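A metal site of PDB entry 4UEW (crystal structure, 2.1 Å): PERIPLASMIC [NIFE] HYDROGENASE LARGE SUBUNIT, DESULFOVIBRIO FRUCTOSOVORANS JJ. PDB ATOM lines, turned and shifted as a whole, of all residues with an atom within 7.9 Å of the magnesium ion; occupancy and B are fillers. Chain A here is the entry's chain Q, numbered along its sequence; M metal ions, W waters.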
ATOM      1  N   GLU A  53     -15.875   1.043  -6.440  1.00  0.00           N
ATOM      2  CA  GLU A  53     -16.101   2.411  -5.944  1.00  0.00           C
ATOM      3  C   GLU A  53     -14.949   2.868  -5.050  1.00  0.00           C
ATOM      4  O   GLU A  53     -14.463   4.007  -5.133  1.00  0.00           O
ATOM      5  CB  GLU A  53     -17.461   2.491  -5.223  1.00  0.00           C
ATOM      6  CG  GLU A  53     -18.659   2.267  -6.175  1.00  0.00           C
ATOM      7  CD  GLU A  53     -19.894   1.743  -5.477  1.00  0.00           C
ATOM      8  OE1 GLU A  53     -19.725   1.129  -4.380  1.00  0.00           O
ATOM      9  OE2 GLU A  53     -21.014   1.915  -6.021  1.00  0.00           O
ATOM     10  N   GLU A 334     -29.888   4.136  -1.650  1.00  0.00           N
ATOM     11  CA  GLU A 334     -29.481   2.789  -1.350  1.00  0.00           C
ATOM     12  C   GLU A 334     -29.408   2.622   0.165  1.00  0.00           C
ATOM     13  O   GLU A 334     -28.877   3.483   0.866  1.00  0.00           O
ATOM     14  CB  GLU A 334     -28.137   2.460  -2.013  1.00  0.00           C
ATOM     15  CG  GLU A 334     -28.188   2.453  -3.550  1.00  0.00           C
ATOM     16  CD  GLU A 334     -26.841   2.166  -4.178  1.00  0.00           C
ATOM     17  OE1 GLU A 334     -25.909   3.017  -4.072  1.00  0.00           O
ATOM     18  OE2 GLU A 334     -26.736   1.104  -4.838  1.00  0.00           O
ATOM     19  N   TYR A 341     -22.228  -4.075   5.038  1.00  0.00           N
ATOM     20  CA  TYR A 341     -21.594  -2.772   5.111  1.00  0.00           C
ATOM     21  C   TYR A 341     -21.771  -2.152   6.484  1.00  0.00           C
ATOM     22  O   TYR A 341     -22.630  -2.552   7.255  1.00  0.00           O
ATOM     23  CB  TYR A 341     -22.121  -1.833   4.021  1.00  0.00           C
ATOM     24  CG  TYR A 341     -21.857  -2.358   2.607  1.00  0.00           C
ATOM     25  CD1 TYR A 341     -20.624  -2.163   1.992  1.00  0.00           C
ATOM     26  CD2 TYR A 341     -22.815  -3.086   1.930  1.00  0.00           C
ATOM     27  CE1 TYR A 341     -20.347  -2.674   0.722  1.00  0.00           C
ATOM     28  CE2 TYR A 341     -22.564  -3.599   0.636  1.00  0.00           C
ATOM     29  CZ  TYR A 341     -21.335  -3.375   0.023  1.00  0.00           C
ATOM     30  OH  TYR A 341     -21.098  -3.906  -1.254  1.00  0.00           O
ATOM     31  N   PRO A 350     -27.080   8.342  -4.313  1.00  0.00           N
ATOM     32  CA  PRO A 350     -25.759   7.929  -4.833  1.00  0.00           C
ATOM     33  C   PRO A 350     -24.699   9.038  -4.870  1.00  0.00           C
ATOM     34  O   PRO A 350     -23.507   8.742  -4.690  1.00  0.00           O
ATOM     35  CB  PRO A 350     -26.060   7.403  -6.234  1.00  0.00           C
ATOM     36  CG  PRO A 350     -27.481   6.954  -6.152  1.00  0.00           C
ATOM     37  CD  PRO A 350     -28.190   7.815  -5.126  1.00  0.00           C
ATOM     38  N   GLY A 353     -23.175   8.498  -1.738  1.00  0.00           N
ATOM     39  CA  GLY A 353     -23.000   7.074  -1.456  1.00  0.00           C
ATOM     40  C   GLY A 353     -21.759   6.775  -0.632  1.00  0.00           C
ATOM     41  O   GLY A 353     -20.771   7.501  -0.690  1.00  0.00           O
ATOM     42  N   VAL A 354     -21.843   5.689   0.149  1.00  0.00           N
ATOM     43  CA  VAL A 354     -20.763   5.268   1.053  1.00  0.00           C
ATOM     44  C   VAL A 354     -20.601   3.763   0.871  1.00  0.00           C
ATOM     45  O   VAL A 354     -21.591   3.026   0.857  1.00  0.00           O
ATOM     46  CB  VAL A 354     -21.061   5.640   2.551  1.00  0.00           C
ATOM     47  CG1 VAL A 354     -19.968   5.119   3.469  1.00  0.00           C
ATOM     48  CG2 VAL A 354     -21.173   7.155   2.680  1.00  0.00           C
ATOM     49  N   THR A 355     -19.355   3.334   0.672  1.00  0.00           N
ATOM     50  CA  THR A 355     -19.043   1.925   0.458  1.00  0.00           C
ATOM     51  C   THR A 355     -17.992   1.527   1.491  1.00  0.00           C
ATOM     52  O   THR A 355     -16.788   1.728   1.309  1.00  0.00           O
ATOM     53  CB  THR A 355     -18.595   1.658  -0.981  1.00  0.00           C
ATOM     54  OG1 THR A 355     -19.604   2.176  -1.877  1.00  0.00           O
ATOM     55  CG2 THR A 355     -18.366   0.138  -1.216  1.00  0.00           C
ATOM     56  N   TRP A 370     -23.659  -8.889  -0.282  1.00  0.00           N
ATOM     57  CA  TRP A 370     -22.688  -7.867  -0.652  1.00  0.00           C
ATOM     58  C   TRP A 370     -23.335  -6.745  -1.500  1.00  0.00           C
ATOM     59  O   TRP A 370     -22.735  -5.682  -1.695  1.00  0.00           O
ATOM     60  CB  TRP A 370     -21.464  -8.477  -1.354  1.00  0.00           C
ATOM     61  CG  TRP A 370     -20.455  -9.121  -0.387  1.00  0.00           C
ATOM     62  CD1 TRP A 370     -20.162 -10.437  -0.273  1.00  0.00           C
ATOM     63  CD2 TRP A 370     -19.633  -8.431   0.562  1.00  0.00           C
ATOM     64  NE1 TRP A 370     -19.196 -10.637   0.704  1.00  0.00           N
ATOM     65  CE2 TRP A 370     -18.871  -9.417   1.234  1.00  0.00           C
ATOM     66  CE3 TRP A 370     -19.467  -7.088   0.927  1.00  0.00           C
ATOM     67  CZ2 TRP A 370     -17.940  -9.093   2.239  1.00  0.00           C
ATOM     68  CZ3 TRP A 370     -18.557  -6.760   1.920  1.00  0.00           C
ATOM     69  CH2 TRP A 370     -17.788  -7.757   2.551  1.00  0.00           C
ATOM     70  N   MET A 371     -24.576  -6.977  -1.963  1.00  0.00           N
ATOM     71  CA  MET A 371     -25.319  -5.881  -2.623  1.00  0.00           C
ATOM     72  C   MET A 371     -25.962  -4.946  -1.581  1.00  0.00           C
ATOM     73  O   MET A 371     -26.359  -5.386  -0.528  1.00  0.00           O
ATOM     74  CB  MET A 371     -26.400  -6.432  -3.566  1.00  0.00           C
ATOM     75  CG  MET A 371     -25.828  -7.099  -4.828  1.00  0.00           C
ATOM     76  SD  MET A 371     -27.185  -7.532  -5.921  1.00  0.00           S
ATOM     77  CE  MET A 371     -26.419  -8.800  -6.942  1.00  0.00           C
ATOM     78  N   LYS A 372     -25.998  -3.642  -1.905  1.00  0.00           N
ATOM     79  CA  LYS A 372     -26.791  -2.659  -1.204  1.00  0.00           C
ATOM     80  C   LYS A 372     -28.206  -2.908  -1.692  1.00  0.00           C
ATOM     81  O   LYS A 372     -28.393  -3.759  -2.537  1.00  0.00           O
ATOM     82  CB  LYS A 372     -26.346  -1.251  -1.565  1.00  0.00           C
ATOM     83  CG  LYS A 372     -24.880  -0.954  -1.268  1.00  0.00           C
ATOM     84  CD  LYS A 372     -24.500   0.482  -1.655  1.00  0.00           C
ATOM     85  CE  LYS A 372     -23.164   0.855  -1.046  1.00  0.00           C
ATOM     86  NZ  LYS A 372     -22.623   2.060  -1.714  1.00  0.00           N
ATOM     87  N   PRO A 374     -31.122  -0.799  -3.328  1.00  0.00           N
ATOM     88  CA  PRO A 374     -31.632   0.449  -3.913  1.00  0.00           C
ATOM     89  C   PRO A 374     -33.135   0.513  -3.770  1.00  0.00           C
ATOM     90  O   PRO A 374     -33.813  -0.494  -3.976  1.00  0.00           O
ATOM     91  CB  PRO A 374     -31.281   0.329  -5.424  1.00  0.00           C
ATOM     92  CG  PRO A 374     -30.311  -0.792  -5.535  1.00  0.00           C
ATOM     93  CD  PRO A 374     -30.618  -1.719  -4.377  1.00  0.00           C
ATOM     94  N   SER A 480     -27.120   3.443 -13.459  1.00  0.00           N
ATOM     95  CA  SER A 480     -26.605   4.799 -13.267  1.00  0.00           C
ATOM     96  C   SER A 480     -25.230   4.815 -12.581  1.00  0.00           C
ATOM     97  O   SER A 480     -25.002   4.026 -11.662  1.00  0.00           O
ATOM     98  CB  SER A 480     -27.602   5.683 -12.511  1.00  0.00           C
ATOM     99  OG  SER A 480     -28.097   5.042 -11.336  1.00  0.00           O
ATOM    100  N   TRP A 482     -22.550   7.739 -10.879  1.00  0.00           N
ATOM    101  CA  TRP A 482     -22.671   9.059 -10.261  1.00  0.00           C
ATOM    102  C   TRP A 482     -21.323   9.474  -9.728  1.00  0.00           C
ATOM    103  O   TRP A 482     -20.731   8.761  -8.895  1.00  0.00           O
ATOM    104  CB  TRP A 482     -23.653   9.053  -9.090  1.00  0.00           C
ATOM    105  CG  TRP A 482     -25.002   8.369  -9.321  1.00  0.00           C
ATOM    106  CD1 TRP A 482     -25.247   7.036  -9.353  1.00  0.00           C
ATOM    107  CD2 TRP A 482     -26.274   9.014  -9.443  1.00  0.00           C
ATOM    108  NE1 TRP A 482     -26.609   6.810  -9.498  1.00  0.00           N
ATOM    109  CE2 TRP A 482     -27.250   8.001  -9.579  1.00  0.00           C
ATOM    110  CE3 TRP A 482     -26.687  10.364  -9.460  1.00  0.00           C
ATOM    111  CZ2 TRP A 482     -28.614   8.284  -9.754  1.00  0.00           C
ATOM    112  CZ3 TRP A 482     -28.036  10.636  -9.634  1.00  0.00           C
ATOM    113  CH2 TRP A 482     -28.986   9.590  -9.769  1.00  0.00           C
ATOM    114  N   PHE A 493     -17.390   8.001  -6.463  1.00  0.00           N
ATOM    115  CA  PHE A 493     -17.904   7.360  -7.680  1.00  0.00           C
ATOM    116  C   PHE A 493     -18.790   6.185  -7.300  1.00  0.00           C
ATOM    117  O   PHE A 493     -18.336   5.234  -6.678  1.00  0.00           O
ATOM    118  CB  PHE A 493     -16.782   6.937  -8.654  1.00  0.00           C
ATOM    119  CG  PHE A 493     -17.255   6.816 -10.066  1.00  0.00           C
ATOM    120  CD1 PHE A 493     -18.102   5.765 -10.451  1.00  0.00           C
ATOM    121  CD2 PHE A 493     -16.844   7.717 -11.019  1.00  0.00           C
ATOM    122  CE1 PHE A 493     -18.554   5.663 -11.777  1.00  0.00           C
ATOM    123  CE2 PHE A 493     -17.280   7.603 -12.344  1.00  0.00           C
ATOM    124  CZ  PHE A 493     -18.125   6.573 -12.717  1.00  0.00           C
ATOM    125  N   GLN A 494     -20.067   6.269  -7.631  1.00  0.00           N
ATOM    126  CA  GLN A 494     -21.026   5.287  -7.185  1.00  0.00           C
ATOM    127  C   GLN A 494     -21.732   4.659  -8.386  1.00  0.00           C
ATOM    128  O   GLN A 494     -22.251   5.364  -9.261  1.00  0.00           O
ATOM    129  CB  GLN A 494     -22.020   5.914  -6.197  1.00  0.00           C
ATOM    130  CG  GLN A 494     -21.444   6.350  -4.856  1.00  0.00           C
ATOM    131  CD  GLN A 494     -21.038   5.220  -3.890  1.00  0.00           C
ATOM    132  OE1 GLN A 494     -21.724   4.219  -3.753  1.00  0.00           O
ATOM    133  NE2 GLN A 494     -19.904   5.400  -3.193  1.00  0.00           N
ATOM    134  N   LEU A 495     -21.730   3.337  -8.444  1.00  0.00           N
ATOM    135  CA  LEU A 495     -22.555   2.590  -9.408  1.00  0.00           C
ATOM    136  C   LEU A 495     -23.813   2.090  -8.680  1.00  0.00           C
ATOM    137  O   LEU A 495     -23.711   1.641  -7.528  1.00  0.00           O
ATOM    138  CB  LEU A 495     -21.792   1.384  -9.939  1.00  0.00           C
ATOM    139  CG  LEU A 495     -20.490   1.602 -10.745  1.00  0.00           C
ATOM    140  CD1 LEU A 495     -19.309   2.094  -9.884  1.00  0.00           C
ATOM    141  CD2 LEU A 495     -20.072   0.303 -11.432  1.00  0.00           C
ATOM    142  N   VAL A 496     -24.969   2.254  -9.312  1.00  0.00           N
ATOM    143  CA  VAL A 496     -26.238   1.602  -8.942  1.00  0.00           C
ATOM    144  C   VAL A 496     -26.705   0.885 -10.209  1.00  0.00           C
ATOM    145  O   VAL A 496     -27.010   1.515 -11.192  1.00  0.00           O
ATOM    146  CB  VAL A 496     -27.339   2.614  -8.534  1.00  0.00           C
ATOM    147  CG1 VAL A 496     -28.581   1.874  -8.066  1.00  0.00           C
ATOM    148  CG2 VAL A 496     -26.814   3.553  -7.474  1.00  0.00           C
ATOM    149  N   VAL A 497     -26.742  -0.442 -10.150  1.00  0.00           N
ATOM    150  CA  VAL A 497     -26.700  -1.289 -11.318  1.00  0.00           C
ATOM    151  C   VAL A 497     -27.980  -2.107 -11.297  1.00  0.00           C
ATOM    152  O   VAL A 497     -28.479  -2.363 -10.222  1.00  0.00           O
ATOM    153  CB  VAL A 497     -25.437  -2.174 -11.288  1.00  0.00           C
ATOM    154  CG1 VAL A 497     -25.319  -3.011 -12.545  1.00  0.00           C
ATOM    155  CG2 VAL A 497     -24.176  -1.297 -11.144  1.00  0.00           C
ATOM    156  N   THR A 500     -28.516  -4.831  -8.870  1.00  0.00           N
ATOM    157  CA  THR A 500     -28.585  -4.301  -7.509  1.00  0.00           C
ATOM    158  C   THR A 500     -30.057  -4.042  -7.184  1.00  0.00           C
ATOM    159  O   THR A 500     -30.530  -4.395  -6.093  1.00  0.00           O
ATOM    160  CB  THR A 500     -27.775  -3.001  -7.312  1.00  0.00           C
ATOM    161  OG1 THR A 500     -26.558  -3.057  -8.061  1.00  0.00           O
ATOM    162  CG2 THR A 500     -27.413  -2.821  -5.840  1.00  0.00           C
ATOM    163  N   CYS A 546     -21.997  -7.212 -11.532  1.00  0.00           N
ATOM    164  CA  CYS A 546     -22.704  -5.923 -11.756  1.00  0.00           C
ATOM    165  C   CYS A 546     -23.330  -5.439 -10.436  1.00  0.00           C
ATOM    166  O   CYS A 546     -23.065  -4.308 -10.003  1.00  0.00           O
ATOM    167  CB  CYS A 546     -23.815  -6.041 -12.810  1.00  0.00           C
ATOM    168  SG  CYS A 546     -23.267  -5.698 -14.489  1.00  0.00           S
ATOM    169  N   GLY A 547     -24.133  -6.294  -9.806  1.00  0.00           N
ATOM    170  CA  GLY A 547     -24.895  -5.888  -8.611  1.00  0.00           C
ATOM    171  C   GLY A 547     -24.032  -5.390  -7.470  1.00  0.00           C
ATOM    172  O   GLY A 547     -24.401  -4.427  -6.783  1.00  0.00           O
ATOM    173  N   VAL A 548     -22.870  -6.027  -7.291  1.00  0.00           N
ATOM    174  CA  VAL A 548     -21.994  -5.713  -6.153  1.00  0.00           C
ATOM    175  C   VAL A 548     -20.890  -4.718  -6.568  1.00  0.00           C
ATOM    176  O   VAL A 548     -20.612  -3.754  -5.823  1.00  0.00           O
ATOM    177  CB  VAL A 548     -21.331  -6.989  -5.559  1.00  0.00           C
ATOM    178  CG1 VAL A 548     -20.423  -6.629  -4.392  1.00  0.00           C
ATOM    179  CG2 VAL A 548     -22.348  -8.035  -5.146  1.00  0.00           C
ATOM    180  N   HIS A 549     -20.272  -4.947  -7.737  1.00  0.00           N
ATOM    181  CA  HIS A 549     -19.101  -4.179  -8.141  1.00  0.00           C
ATOM    182  C   HIS A 549     -18.074  -3.964  -7.000  1.00  0.00           C
ATOM    183  O   HIS A 549     -17.558  -2.864  -6.718  1.00  0.00           O
ATOM    184  CB  HIS A 549     -19.459  -2.857  -8.842  1.00  0.00           C
ATOM    185  CG  HIS A 549     -20.585  -2.107  -8.206  1.00  0.00           C
ATOM    186  ND1 HIS A 549     -21.902  -2.415  -8.422  1.00  0.00           N
ATOM    187  CD2 HIS A 549     -20.573  -1.069  -7.339  1.00  0.00           C
ATOM    188  CE1 HIS A 549     -22.670  -1.599  -7.732  1.00  0.00           C
ATOM    189  NE2 HIS A 549     -21.885  -0.769  -7.060  1.00  0.00           N
ATOM    190  OXT HIS A 549     -17.703  -4.922  -6.349  1.00  0.00           O
HETATM  191 MG    MG M   1     -22.774   0.830  -5.775  1.00  0.00          MG
HETATM  192  O   HOH W   1     -23.465   2.418  -4.737  1.00  0.00           O
HETATM  193  O   HOH W   2     -21.947   0.000  -4.088  1.00  0.00           O
HETATM  194  O   HOH W   3     -24.487  -0.236  -5.469  1.00  0.00           O
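Water W1 lies within hydrogen-bond range of the side-chain carboxylate of Glu 334 (2.6 Å), the side-chain amide oxygen of Gln 494 (2.7 Å) and the side-chain amino group of Lys 372 (3.2 Å).
Water W2 lies within hydrogen-bond range of OE1 of Glu 53 and NZ of Lys 372.
Water W1 binds the magnesium ion.
The magnesium ion is bound by water W3 (2.0 Å).
Water W2 binds the magnesium ion (2.1 Å).
OE2 of Glu 53 is bound to the magnesium ion (2.1 Å).
O of Leu 495 is bound to the magnesium ion.
NE2 of His 549 is bound to the magnesium ion, at 2.2 Å.
The magnesium ion has six donor atoms within binding distance.
ND1 of His 549 lies within hydrogen-bond range of O of Cys 546.
The side-chain amide oxygen (OE1) of Gln 494 lies close to the side-chain carboxylate (OE2) of Glu 53 (3.3 Å).
OG1 of Thr 355 sits at hydrogen-bond distance from OE1 of Glu 53 (2.7 Å).
Within 4 Å of the magnesium ion: Glu 53, Leu 495 and His 549.
The nearest printed residue that does not touch the magnesium ion is Glu 334 (4.1 Å).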
